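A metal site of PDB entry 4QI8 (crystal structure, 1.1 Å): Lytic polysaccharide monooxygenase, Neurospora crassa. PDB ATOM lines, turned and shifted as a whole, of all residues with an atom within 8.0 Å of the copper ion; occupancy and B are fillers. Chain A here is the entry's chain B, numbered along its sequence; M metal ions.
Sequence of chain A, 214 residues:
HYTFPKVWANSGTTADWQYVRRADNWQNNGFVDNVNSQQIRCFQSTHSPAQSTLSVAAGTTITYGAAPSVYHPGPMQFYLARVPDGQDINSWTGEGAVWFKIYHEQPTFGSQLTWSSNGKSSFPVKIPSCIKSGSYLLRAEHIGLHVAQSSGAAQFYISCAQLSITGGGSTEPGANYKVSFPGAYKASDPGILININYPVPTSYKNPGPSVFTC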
ATOM      1  N   HIS A   1     -11.858  -2.154 -25.031  1.00  0.00           N
ATOM      2  CA  HIS A   1     -10.955  -1.150 -24.487  1.00  0.00           C
ATOM      3  C   HIS A   1     -11.646  -0.165 -23.554  1.00  0.00           C
ATOM      4  O   HIS A   1     -12.380   0.710 -23.983  1.00  0.00           O
ATOM      5  CB  HIS A   1     -10.247  -0.433 -25.629  1.00  0.00           C
ATOM      6  CG  HIS A   1      -9.160  -1.261 -26.205  1.00  0.00           C
ATOM      7  ND1 HIS A   1      -9.396  -2.553 -26.596  1.00  0.00           N
ATOM      8  CD2 HIS A   1      -7.845  -1.037 -26.353  1.00  0.00           C
ATOM      9  CE1 HIS A   1      -8.256  -3.093 -27.009  1.00  0.00           C
ATOM     10  NE2 HIS A   1      -7.298  -2.179 -26.885  1.00  0.00           N
ATOM     11  N   TYR A   2     -11.434  -0.368 -22.262  1.00  0.00           N
ATOM     12  CA  TYR A   2     -12.037   0.460 -21.224  1.00  0.00           C
ATOM     13  C   TYR A   2     -11.211   0.271 -19.968  1.00  0.00           C
ATOM     14  O   TYR A   2     -10.569  -0.764 -19.778  1.00  0.00           O
ATOM     15  CB  TYR A   2     -13.525   0.116 -20.966  1.00  0.00           C
ATOM     16  CG  TYR A   2     -13.887  -1.292 -21.334  1.00  0.00           C
ATOM     17  CD1 TYR A   2     -14.387  -1.579 -22.581  1.00  0.00           C
ATOM     18  CD2 TYR A   2     -13.708  -2.347 -20.435  1.00  0.00           C
ATOM     19  CE1 TYR A   2     -14.681  -2.888 -22.961  1.00  0.00           C
ATOM     20  CE2 TYR A   2     -14.000  -3.660 -20.802  1.00  0.00           C
ATOM     21  CZ  TYR A   2     -14.484  -3.917 -22.073  1.00  0.00           C
ATOM     22  OH  TYR A   2     -14.763  -5.193 -22.490  1.00  0.00           O
ATOM     23  N   ASN A  28      -4.067   3.960 -22.474  1.00  0.00           N
ATOM     24  CA  ASN A  28      -4.222   3.176 -23.698  1.00  0.00           C
ATOM     25  C   ASN A  28      -5.480   2.325 -23.753  1.00  0.00           C
ATOM     26  O   ASN A  28      -5.828   1.865 -24.841  1.00  0.00           O
ATOM     27  CB  ASN A  28      -2.947   2.373 -24.006  1.00  0.00           C
ATOM     28  CG  ASN A  28      -2.571   1.406 -22.903  1.00  0.00           C
ATOM     29  OD1 ASN A  28      -3.388   0.622 -22.425  1.00  0.00           O
ATOM     30  ND2 ASN A  28      -1.299   1.456 -22.492  1.00  0.00           N
ATOM     31  N   ASN A  29      -6.161   2.142 -22.619  1.00  0.00           N
ATOM     32  CA  ASN A  29      -7.375   1.335 -22.533  1.00  0.00           C
ATOM     33  C   ASN A  29      -7.223  -0.143 -22.894  1.00  0.00           C
ATOM     34  O   ASN A  29      -8.210  -0.855 -23.053  1.00  0.00           O
ATOM     35  CB  ASN A  29      -8.509   1.933 -23.374  1.00  0.00           C
ATOM     36  CG  ASN A  29      -8.989   3.252 -22.846  1.00  0.00           C
ATOM     37  OD1 ASN A  29      -9.126   3.438 -21.651  1.00  0.00           O
ATOM     38  ND2 ASN A  29      -9.262   4.186 -23.758  1.00  0.00           N
ATOM     39  N   GLY A  30      -5.978  -0.603 -22.981  1.00  0.00           N
ATOM     40  CA  GLY A  30      -5.692  -1.967 -23.381  1.00  0.00           C
ATOM     41  C   GLY A  30      -5.928  -2.979 -22.274  1.00  0.00           C
ATOM     42  O   GLY A  30      -6.492  -2.692 -21.218  1.00  0.00           O
ATOM     43  N   PHE A  31      -5.517  -4.210 -22.559  1.00  0.00           N
ATOM     44  CA  PHE A  31      -5.868  -5.372 -21.760  1.00  0.00           C
ATOM     45  C   PHE A  31      -4.637  -6.189 -21.412  1.00  0.00           C
ATOM     46  O   PHE A  31      -3.576  -6.061 -22.016  1.00  0.00           O
ATOM     47  CB  PHE A  31      -6.874  -6.266 -22.525  1.00  0.00           C
ATOM     48  CG  PHE A  31      -6.416  -6.629 -23.922  1.00  0.00           C
ATOM     49  CD1 PHE A  31      -5.538  -7.672 -24.134  1.00  0.00           C
ATOM     50  CD2 PHE A  31      -6.828  -5.878 -25.014  1.00  0.00           C
ATOM     51  CE1 PHE A  31      -5.095  -7.985 -25.404  1.00  0.00           C
ATOM     52  CE2 PHE A  31      -6.375  -6.194 -26.285  1.00  0.00           C
ATOM     53  CZ  PHE A  31      -5.505  -7.238 -26.482  1.00  0.00           C
ATOM     54  N   TYR A  71     -18.227  -2.790 -23.815  1.00  0.00           N
ATOM     55  CA  TYR A  71     -18.862  -3.055 -25.110  1.00  0.00           C
ATOM     56  C   TYR A  71     -18.320  -4.325 -25.767  1.00  0.00           C
ATOM     57  O   TYR A  71     -18.768  -4.648 -26.847  1.00  0.00           O
ATOM     58  CB  TYR A  71     -18.750  -1.840 -26.059  1.00  0.00           C
ATOM     59  CG  TYR A  71     -17.329  -1.505 -26.391  1.00  0.00           C
ATOM     60  CD1 TYR A  71     -16.685  -2.069 -27.494  1.00  0.00           C
ATOM     61  CD2 TYR A  71     -16.602  -0.646 -25.587  1.00  0.00           C
ATOM     62  CE1 TYR A  71     -15.349  -1.796 -27.765  1.00  0.00           C
ATOM     63  CE2 TYR A  71     -15.286  -0.374 -25.848  1.00  0.00           C
ATOM     64  CZ  TYR A  71     -14.655  -0.951 -26.938  1.00  0.00           C
ATOM     65  OH  TYR A  71     -13.332  -0.650 -27.131  1.00  0.00           O
ATOM     66  N   HIS A  72     -17.373  -5.028 -25.151  1.00  0.00           N
ATOM     67  CA  HIS A  72     -16.995  -6.337 -25.661  1.00  0.00           C
ATOM     68  C   HIS A  72     -17.831  -7.398 -24.924  1.00  0.00           C
ATOM     69  O   HIS A  72     -18.162  -7.217 -23.746  1.00  0.00           O
ATOM     70  CB  HIS A  72     -15.516  -6.655 -25.393  1.00  0.00           C
ATOM     71  CG  HIS A  72     -14.533  -5.755 -26.086  1.00  0.00           C
ATOM     72  ND1 HIS A  72     -14.516  -5.567 -27.453  1.00  0.00           N
ATOM     73  CD2 HIS A  72     -13.455  -5.084 -25.603  1.00  0.00           C
ATOM     74  CE1 HIS A  72     -13.483  -4.787 -27.772  1.00  0.00           C
ATOM     75  NE2 HIS A  72     -12.819  -4.494 -26.667  1.00  0.00           N
ATOM     76  N   GLY A 144     -13.092  -9.916 -22.077  1.00  0.00           N
ATOM     77  CA  GLY A 144     -13.590  -9.787 -23.429  1.00  0.00           C
ATOM     78  C   GLY A 144     -13.266 -11.041 -24.227  1.00  0.00           C
ATOM     79  O   GLY A 144     -12.097 -11.421 -24.384  1.00  0.00           O
ATOM     80  N   HIS A 146     -14.591 -11.911 -27.455  1.00  0.00           N
ATOM     81  CA  HIS A 146     -14.938 -11.825 -28.879  1.00  0.00           C
ATOM     82  C   HIS A 146     -13.955 -12.524 -29.834  1.00  0.00           C
ATOM     83  O   HIS A 146     -14.369 -12.935 -30.906  1.00  0.00           O
ATOM     84  CB  HIS A 146     -15.172 -10.376 -29.301  1.00  0.00           C
ATOM     85  CG  HIS A 146     -14.093  -9.431 -28.882  1.00  0.00           C
ATOM     86  ND1 HIS A 146     -13.821  -9.187 -27.554  1.00  0.00           N
ATOM     87  CD2 HIS A 146     -13.228  -8.679 -29.600  1.00  0.00           C
ATOM     88  CE1 HIS A 146     -12.811  -8.331 -27.484  1.00  0.00           C
ATOM     89  NE2 HIS A 146     -12.441  -8.007 -28.709  1.00  0.00           N
ATOM     90  N   GLN A 155      -9.263 -11.088 -23.517  1.00  0.00           N
ATOM     91  CA  GLN A 155      -8.790  -9.751 -23.126  1.00  0.00           C
ATOM     92  C   GLN A 155      -9.270  -9.418 -21.727  1.00  0.00           C
ATOM     93  O   GLN A 155     -10.482  -9.290 -21.487  1.00  0.00           O
ATOM     94  CB  GLN A 155      -9.312  -8.719 -24.121  1.00  0.00           C
ATOM     95  CG  GLN A 155      -8.771  -8.921 -25.522  1.00  0.00           C
ATOM     96  CD  GLN A 155      -9.382  -7.986 -26.546  1.00  0.00           C
ATOM     97  OE1 GLN A 155     -10.259  -7.155 -26.231  1.00  0.00           O
ATOM     98  NE2 GLN A 155      -8.949  -8.120 -27.785  1.00  0.00           N
ATOM     99  N   TYR A 157      -9.617  -6.847 -18.716  1.00  0.00           N
ATOM    100  CA  TYR A 157      -9.634  -5.434 -18.371  1.00  0.00           C
ATOM    101  C   TYR A 157      -9.863  -5.353 -16.866  1.00  0.00           C
ATOM    102  O   TYR A 157     -10.914  -5.776 -16.376  1.00  0.00           O
ATOM    103  CB  TYR A 157     -10.769  -4.728 -19.123  1.00  0.00           C
ATOM    104  CG  TYR A 157     -10.614  -4.798 -20.636  1.00  0.00           C
ATOM    105  CD1 TYR A 157      -9.832  -3.883 -21.317  1.00  0.00           C
ATOM    106  CD2 TYR A 157     -11.244  -5.793 -21.374  1.00  0.00           C
ATOM    107  CE1 TYR A 157      -9.673  -3.943 -22.702  1.00  0.00           C
ATOM    108  CE2 TYR A 157     -11.109  -5.858 -22.757  1.00  0.00           C
ATOM    109  CZ  TYR A 157     -10.317  -4.939 -23.409  1.00  0.00           C
ATOM    110  OH  TYR A 157     -10.156  -4.969 -24.786  1.00  0.00           O
HETATM  111 CU    CU M   1     -11.158  -3.406 -26.598  1.00  0.00          CU
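OH of Tyr 71 sits close to N of His 1 (3.0 Å). A ring nitrogen (NE2) of His 146 lies close to a ring nitrogen (ND1) of His 72, at 3.4 Å. A ring nitrogen (NE2) of His 146 lies close to the side-chain amide oxygen (OE1) of Gln 155, at 3.4 Å. The backbone carbonyl oxygen of Gln 155 is in hydrogen-bond range of the backbone NH of Gly 144 (2.7 Å). OE1 of Gln 155 lies close to OH of Tyr 157.
Residues that only touch the copper ion: Tyr 71 and Gln 155.
The copper ion is bound by a ring nitrogen (ND1) of His 1 (2.0 Å), a ring nitrogen (NE2) of His 72 (2.0 Å), the backbone nitrogen (N) of His 1 (2.1 Å) and the side-chain hydroxyl (OH) of Tyr 157 (2.6 Å).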
